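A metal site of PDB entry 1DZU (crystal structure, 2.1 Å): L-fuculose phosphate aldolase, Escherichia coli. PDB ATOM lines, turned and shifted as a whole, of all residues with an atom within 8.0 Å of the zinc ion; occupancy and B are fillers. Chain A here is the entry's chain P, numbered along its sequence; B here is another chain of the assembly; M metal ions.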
ATOM      1  N   ALA A  27     -17.744 -11.070   5.225  1.00  0.00           N
ATOM      2  CA  ALA A  27     -16.694 -11.957   4.781  1.00  0.00           C
ATOM      3  C   ALA A  27     -15.408 -11.292   4.359  1.00  0.00           C
ATOM      4  O   ALA A  27     -14.402 -11.977   4.126  1.00  0.00           O
ATOM      5  CB  ALA A  27     -17.289 -12.729   3.597  1.00  0.00           C
ATOM      6  N   GLY A  28     -15.397  -9.979   4.231  1.00  0.00           N
ATOM      7  CA  GLY A  28     -14.197  -9.316   3.723  1.00  0.00           C
ATOM      8  C   GLY A  28     -13.036  -9.241   4.684  1.00  0.00           C
ATOM      9  O   GLY A  28     -13.063  -9.454   5.888  1.00  0.00           O
ATOM     10  N   ASN A  29     -11.894  -8.922   4.067  1.00  0.00           N
ATOM     11  CA  ASN A  29     -10.651  -8.763   4.821  1.00  0.00           C
ATOM     12  C   ASN A  29      -9.767  -7.834   3.997  1.00  0.00           C
ATOM     13  O   ASN A  29      -9.879  -7.784   2.787  1.00  0.00           O
ATOM     14  CB  ASN A  29      -9.963 -10.085   5.125  1.00  0.00           C
ATOM     15  CG  ASN A  29     -10.146 -11.166   4.101  1.00  0.00           C
ATOM     16  OD1 ASN A  29      -9.505 -11.156   3.056  1.00  0.00           O
ATOM     17  ND2 ASN A  29     -11.070 -12.065   4.444  1.00  0.00           N
ATOM     18  N   SER A  71      -6.887 -12.895   9.762  1.00  0.00           N
ATOM     19  CA  SER A  71      -7.935 -13.423   8.906  1.00  0.00           C
ATOM     20  C   SER A  71      -7.647 -14.857   8.502  1.00  0.00           C
ATOM     21  O   SER A  71      -6.498 -15.208   8.170  1.00  0.00           O
ATOM     22  CB  SER A  71      -7.931 -12.610   7.586  1.00  0.00           C
ATOM     23  OG  SER A  71      -8.852 -13.166   6.687  1.00  0.00           O
ATOM     24  N   SER A  72      -8.723 -15.666   8.326  1.00  0.00           N
ATOM     25  CA  SER A  72      -8.530 -17.038   7.864  1.00  0.00           C
ATOM     26  C   SER A  72      -8.050 -17.038   6.425  1.00  0.00           C
ATOM     27  O   SER A  72      -7.524 -18.060   5.968  1.00  0.00           O
ATOM     28  CB  SER A  72      -9.861 -17.805   8.011  1.00  0.00           C
ATOM     29  OG  SER A  72     -10.789 -17.166   7.101  1.00  0.00           O
ATOM     30  N   GLU A  73      -8.155 -15.901   5.715  1.00  0.00           N
ATOM     31  CA  GLU A  73      -7.673 -15.823   4.342  1.00  0.00           C
ATOM     32  C   GLU A  73      -6.389 -15.013   4.195  1.00  0.00           C
ATOM     33  O   GLU A  73      -6.098 -14.515   3.105  1.00  0.00           O
ATOM     34  CB  GLU A  73      -8.781 -15.238   3.437  1.00  0.00           C
ATOM     35  CG  GLU A  73     -10.146 -15.844   3.760  1.00  0.00           C
ATOM     36  CD  GLU A  73     -11.132 -15.740   2.624  1.00  0.00           C
ATOM     37  OE1 GLU A  73     -10.933 -16.414   1.600  1.00  0.00           O
ATOM     38  OE2 GLU A  73     -12.144 -15.035   2.749  1.00  0.00           O
ATOM     39  N   PHE A  76      -3.455 -15.589   0.879  1.00  0.00           N
ATOM     40  CA  PHE A  76      -3.428 -15.038  -0.478  1.00  0.00           C
ATOM     41  C   PHE A  76      -3.169 -13.530  -0.438  1.00  0.00           C
ATOM     42  O   PHE A  76      -2.772 -12.997  -1.474  1.00  0.00           O
ATOM     43  CB  PHE A  76      -4.604 -15.439  -1.361  1.00  0.00           C
ATOM     44  CG  PHE A  76      -6.000 -15.112  -0.942  1.00  0.00           C
ATOM     45  CD1 PHE A  76      -6.352 -13.877  -0.423  1.00  0.00           C
ATOM     46  CD2 PHE A  76      -6.997 -16.075  -1.071  1.00  0.00           C
ATOM     47  CE1 PHE A  76      -7.659 -13.616  -0.047  1.00  0.00           C
ATOM     48  CE2 PHE A  76      -8.303 -15.831  -0.681  1.00  0.00           C
ATOM     49  CZ  PHE A  76      -8.652 -14.590  -0.168  1.00  0.00           C
ATOM     50  N   HIS A  77      -3.315 -12.826   0.682  1.00  0.00           N
ATOM     51  CA  HIS A  77      -2.898 -11.431   0.797  1.00  0.00           C
ATOM     52  C   HIS A  77      -1.370 -11.438   0.650  1.00  0.00           C
ATOM     53  O   HIS A  77      -0.884 -10.564  -0.056  1.00  0.00           O
ATOM     54  CB  HIS A  77      -3.220 -10.724   2.124  1.00  0.00           C
ATOM     55  CG  HIS A  77      -4.684 -10.451   2.272  1.00  0.00           C
ATOM     56  ND1 HIS A  77      -5.201  -9.175   2.354  1.00  0.00           N
ATOM     57  CD2 HIS A  77      -5.737 -11.317   2.271  1.00  0.00           C
ATOM     58  CE1 HIS A  77      -6.519  -9.245   2.429  1.00  0.00           C
ATOM     59  NE2 HIS A  77      -6.867 -10.542   2.363  1.00  0.00           N
ATOM     60  N   HIS A  92     -10.247  -7.762  -0.239  1.00  0.00           N
ATOM     61  CA  HIS A  92     -10.912  -8.993  -0.624  1.00  0.00           C
ATOM     62  C   HIS A  92     -12.333  -8.975  -0.085  1.00  0.00           C
ATOM     63  O   HIS A  92     -12.534  -8.693   1.098  1.00  0.00           O
ATOM     64  CB  HIS A  92     -10.145 -10.206  -0.031  1.00  0.00           C
ATOM     65  CG  HIS A  92     -10.874 -11.492  -0.184  1.00  0.00           C
ATOM     66  ND1 HIS A  92     -11.265 -12.018  -1.393  1.00  0.00           N
ATOM     67  CD2 HIS A  92     -11.328 -12.362   0.751  1.00  0.00           C
ATOM     68  CE1 HIS A  92     -11.905 -13.151  -1.191  1.00  0.00           C
ATOM     69  NE2 HIS A  92     -11.950 -13.389   0.118  1.00  0.00           N
ATOM     70  N   ASN A  93     -13.311  -9.341  -0.933  1.00  0.00           N
ATOM     71  CA  ASN A  93     -14.662  -9.409  -0.376  1.00  0.00           C
ATOM     72  C   ASN A  93     -15.403 -10.491  -1.109  1.00  0.00           C
ATOM     73  O   ASN A  93     -14.864 -11.048  -2.066  1.00  0.00           O
ATOM     74  CB  ASN A  93     -15.361  -8.068  -0.496  1.00  0.00           C
ATOM     75  CG  ASN A  93     -15.468  -7.604  -1.949  1.00  0.00           C
ATOM     76  OD1 ASN A  93     -15.828  -8.324  -2.869  1.00  0.00           O
ATOM     77  ND2 ASN A  93     -15.109  -6.334  -2.154  1.00  0.00           N
ATOM     78  N   HIS A  94     -16.634 -10.744  -0.714  1.00  0.00           N
ATOM     79  CA  HIS A  94     -17.484 -11.700  -1.385  1.00  0.00           C
ATOM     80  C   HIS A  94     -18.665 -10.918  -1.976  1.00  0.00           C
ATOM     81  O   HIS A  94     -19.810 -11.361  -1.943  1.00  0.00           O
ATOM     82  CB  HIS A  94     -17.917 -12.825  -0.465  1.00  0.00           C
ATOM     83  CG  HIS A  94     -16.856 -13.695   0.147  1.00  0.00           C
ATOM     84  ND1 HIS A  94     -17.169 -14.714   1.032  1.00  0.00           N
ATOM     85  CD2 HIS A  94     -15.495 -13.734   0.050  1.00  0.00           C
ATOM     86  CE1 HIS A  94     -16.046 -15.322   1.437  1.00  0.00           C
ATOM     87  NE2 HIS A  94     -15.022 -14.738   0.847  1.00  0.00           N
ATOM     88  N   PHE A 131     -10.353 -22.485   0.468  1.00  0.00           N
ATOM     89  CA  PHE A 131      -9.910 -21.248   1.080  1.00  0.00           C
ATOM     90  C   PHE A 131      -8.725 -21.539   2.040  1.00  0.00           C
ATOM     91  O   PHE A 131      -8.625 -22.670   2.534  1.00  0.00           O
ATOM     92  CB  PHE A 131     -11.035 -20.512   1.839  1.00  0.00           C
ATOM     93  CG  PHE A 131     -11.444 -21.148   3.137  1.00  0.00           C
ATOM     94  CD1 PHE A 131     -12.333 -22.217   3.139  1.00  0.00           C
ATOM     95  CD2 PHE A 131     -10.924 -20.709   4.338  1.00  0.00           C
ATOM     96  CE1 PHE A 131     -12.723 -22.828   4.318  1.00  0.00           C
ATOM     97  CE2 PHE A 131     -11.301 -21.311   5.533  1.00  0.00           C
ATOM     98  CZ  PHE A 131     -12.202 -22.365   5.513  1.00  0.00           C
ATOM     99  N   GLY A 132      -7.809 -20.597   2.204  1.00  0.00           N
ATOM    100  CA  GLY A 132      -6.696 -20.774   3.110  1.00  0.00           C
ATOM    101  C   GLY A 132      -5.625 -21.738   2.661  1.00  0.00           C
ATOM    102  O   GLY A 132      -4.652 -21.917   3.399  1.00  0.00           O
ATOM    103  N   LEU A 136      -4.741 -22.305  -3.525  1.00  0.00           N
ATOM    104  CA  LEU A 136      -5.503 -21.103  -3.844  1.00  0.00           C
ATOM    105  C   LEU A 136      -4.535 -19.928  -4.033  1.00  0.00           C
ATOM    106  O   LEU A 136      -4.583 -19.214  -5.034  1.00  0.00           O
ATOM    107  CB  LEU A 136      -6.562 -20.756  -2.786  1.00  0.00           C
ATOM    108  CG  LEU A 136      -7.443 -19.543  -3.090  1.00  0.00           C
ATOM    109  CD1 LEU A 136      -8.050 -19.609  -4.494  1.00  0.00           C
ATOM    110  CD2 LEU A 136      -8.507 -19.372  -2.014  1.00  0.00           C
ATOM    111  N   LEU A 152     -12.456 -14.973  -8.002  1.00  0.00           N
ATOM    112  CA  LEU A 152     -11.965 -16.302  -7.530  1.00  0.00           C
ATOM    113  C   LEU A 152     -13.157 -17.230  -7.728  1.00  0.00           C
ATOM    114  O   LEU A 152     -14.218 -16.904  -7.194  1.00  0.00           O
ATOM    115  CB  LEU A 152     -11.534 -16.248  -6.092  1.00  0.00           C
ATOM    116  CG  LEU A 152     -10.223 -15.702  -5.571  1.00  0.00           C
ATOM    117  CD1 LEU A 152      -9.788 -14.395  -6.208  1.00  0.00           C
ATOM    118  CD2 LEU A 152     -10.330 -15.437  -4.064  1.00  0.00           C
ATOM    119  N   HIS A 154     -16.262 -19.649  -7.495  1.00  0.00           N
ATOM    120  CA  HIS A 154     -17.085 -20.059  -6.366  1.00  0.00           C
ATOM    121  C   HIS A 154     -16.709 -19.341  -5.077  1.00  0.00           C
ATOM    122  O   HIS A 154     -16.744 -19.958  -3.981  1.00  0.00           O
ATOM    123  CB  HIS A 154     -16.987 -21.578  -6.115  1.00  0.00           C
ATOM    124  CG  HIS A 154     -17.736 -22.326  -7.167  1.00  0.00           C
ATOM    125  ND1 HIS A 154     -19.106 -22.263  -7.286  1.00  0.00           N
ATOM    126  CD2 HIS A 154     -17.288 -23.126  -8.165  1.00  0.00           C
ATOM    127  CE1 HIS A 154     -19.472 -22.993  -8.329  1.00  0.00           C
ATOM    128  NE2 HIS A 154     -18.397 -23.516  -8.885  1.00  0.00           N
ATOM    129  N   HIS A 155     -16.314 -18.049  -5.175  1.00  0.00           N
ATOM    130  CA  HIS A 155     -15.737 -17.457  -3.969  1.00  0.00           C
ATOM    131  C   HIS A 155     -15.922 -15.961  -3.891  1.00  0.00           C
ATOM    132  O   HIS A 155     -16.700 -15.542  -3.005  1.00  0.00           O
ATOM    133  CB  HIS A 155     -14.253 -17.864  -3.929  1.00  0.00           C
ATOM    134  CG  HIS A 155     -13.566 -17.448  -2.664  1.00  0.00           C
ATOM    135  ND1 HIS A 155     -12.631 -18.220  -2.028  1.00  0.00           N
ATOM    136  CD2 HIS A 155     -13.715 -16.350  -1.861  1.00  0.00           C
ATOM    137  CE1 HIS A 155     -12.222 -17.646  -0.930  1.00  0.00           C
ATOM    138  NE2 HIS A 155     -12.847 -16.491  -0.789  1.00  0.00           N
ATOM    139  N   GLY A 156     -15.217 -15.174  -4.690  1.00  0.00           N
ATOM    140  CA  GLY A 156     -15.330 -13.722  -4.564  1.00  0.00           C
ATOM    141  C   GLY A 156     -14.311 -12.918  -5.338  1.00  0.00           C
ATOM    142  O   GLY A 156     -14.013 -13.244  -6.490  1.00  0.00           O
ATOM    143  N   LEU A 157     -13.823 -11.848  -4.713  1.00  0.00           N
ATOM    144  CA  LEU A 157     -12.908 -10.928  -5.417  1.00  0.00           C
ATOM    145  C   LEU A 157     -11.691 -10.549  -4.578  1.00  0.00           C
ATOM    146  O   LEU A 157     -11.810 -10.438  -3.348  1.00  0.00           O
ATOM    147  CB  LEU A 157     -13.737  -9.694  -5.776  1.00  0.00           C
ATOM    148  CG  LEU A 157     -13.353  -8.355  -6.349  1.00  0.00           C
ATOM    149  CD1 LEU A 157     -12.544  -7.531  -5.386  1.00  0.00           C
ATOM    150  CD2 LEU A 157     -12.576  -8.410  -7.658  1.00  0.00           C
ATOM    151  N   ILE A 158     -10.571 -10.276  -5.257  1.00  0.00           N
ATOM    152  CA  ILE A 158      -9.341  -9.736  -4.729  1.00  0.00           C
ATOM    153  C   ILE A 158      -8.956  -8.531  -5.612  1.00  0.00           C
ATOM    154  O   ILE A 158      -8.864  -8.653  -6.839  1.00  0.00           O
ATOM    155  CB  ILE A 158      -8.128 -10.656  -4.636  1.00  0.00           C
ATOM    156  CG1 ILE A 158      -8.483 -12.030  -4.066  1.00  0.00           C
ATOM    157  CG2 ILE A 158      -7.052  -9.992  -3.781  1.00  0.00           C
ATOM    158  CD1 ILE A 158      -7.388 -13.060  -4.160  1.00  0.00           C
ATOM    159  N   HIS B 112     -21.569 -21.991  -3.628  1.00  0.00           N
ATOM    160  CA  HIS B 112     -20.557 -21.226  -2.911  1.00  0.00           C
ATOM    161  C   HIS B 112     -20.094 -22.017  -1.682  1.00  0.00           C
ATOM    162  O   HIS B 112     -20.938 -22.659  -1.055  1.00  0.00           O
ATOM    163  CB  HIS B 112     -21.131 -19.907  -2.429  1.00  0.00           C
ATOM    164  CG  HIS B 112     -20.058 -18.941  -2.014  1.00  0.00           C
ATOM    165  ND1 HIS B 112     -19.456 -18.967  -0.756  1.00  0.00           N
ATOM    166  CD2 HIS B 112     -19.493 -17.932  -2.705  1.00  0.00           C
ATOM    167  CE1 HIS B 112     -18.550 -18.018  -0.715  1.00  0.00           C
ATOM    168  NE2 HIS B 112     -18.546 -17.373  -1.880  1.00  0.00           N
ATOM    169  N   TYR B 113     -18.811 -21.887  -1.310  1.00  0.00           N
ATOM    170  CA  TYR B 113     -18.350 -22.662  -0.160  1.00  0.00           C
ATOM    171  C   TYR B 113     -18.977 -22.269   1.153  1.00  0.00           C
ATOM    172  O   TYR B 113     -18.978 -23.131   2.050  1.00  0.00           O
ATOM    173  CB  TYR B 113     -16.830 -22.706  -0.022  1.00  0.00           C
ATOM    174  CG  TYR B 113     -16.212 -21.435   0.485  1.00  0.00           C
ATOM    175  CD1 TYR B 113     -15.838 -20.427  -0.389  1.00  0.00           C
ATOM    176  CD2 TYR B 113     -16.005 -21.262   1.858  1.00  0.00           C
ATOM    177  CE1 TYR B 113     -15.276 -19.245   0.085  1.00  0.00           C
ATOM    178  CE2 TYR B 113     -15.435 -20.089   2.326  1.00  0.00           C
ATOM    179  CZ  TYR B 113     -15.067 -19.095   1.451  1.00  0.00           C
ATOM    180  OH  TYR B 113     -14.494 -17.939   1.919  1.00  0.00           O
ATOM    181  N   MET B 114     -19.545 -21.096   1.333  1.00  0.00           N
ATOM    182  CA  MET B 114     -20.175 -20.647   2.545  1.00  0.00           C
ATOM    183  C   MET B 114     -21.485 -21.366   2.832  1.00  0.00           C
ATOM    184  O   MET B 114     -21.972 -21.390   3.976  1.00  0.00           O
ATOM    185  CB  MET B 114     -20.371 -19.124   2.629  1.00  0.00           C
ATOM    186  CG  MET B 114     -19.105 -18.344   2.988  1.00  0.00           C
ATOM    187  SD  MET B 114     -18.407 -18.715   4.608  1.00  0.00           S
ATOM    188  CE  MET B 114     -19.857 -18.676   5.652  1.00  0.00           C
HETATM  189 ZN    ZN M   1     -13.005 -15.091   0.821  1.00  0.00          ZN
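Merely in contact with the zinc ion: Tyr 113 of chain B.
Within 4 Å of the zinc ion: Glu 73, His 92, His 94, His 155 and Tyr 113 of chain B.
The zinc ion is bound by NE2 of His 94 (2.0 Å), OE2 of Glu 73 (2.1 Å), NE2 of His 92 (2.1 Å), NE2 of His 155 (2.1 Å) and OE1 of Glu 73 (2.6 Å).
NE2 of His 94 lies close to OH of Tyr 113 of chain B (3.4 Å).
N of Glu 73 sits at hydrogen-bond distance from OG of Ser 71.
O of His 92 is in hydrogen-bond range of N of Asn 29, 3.0 Å away.
O of Leu 157 lies within hydrogen-bond range of ND1 of His 92, at 2.6 Å.
The side-chain hydroxyl (OH) of Tyr 113 of chain B sits close to a ring nitrogen (NE2) of His 155, 3.5 Å away.
NE2 of His 112 of chain B is in hydrogen-bond range of O of His 155 (2.8 Å).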
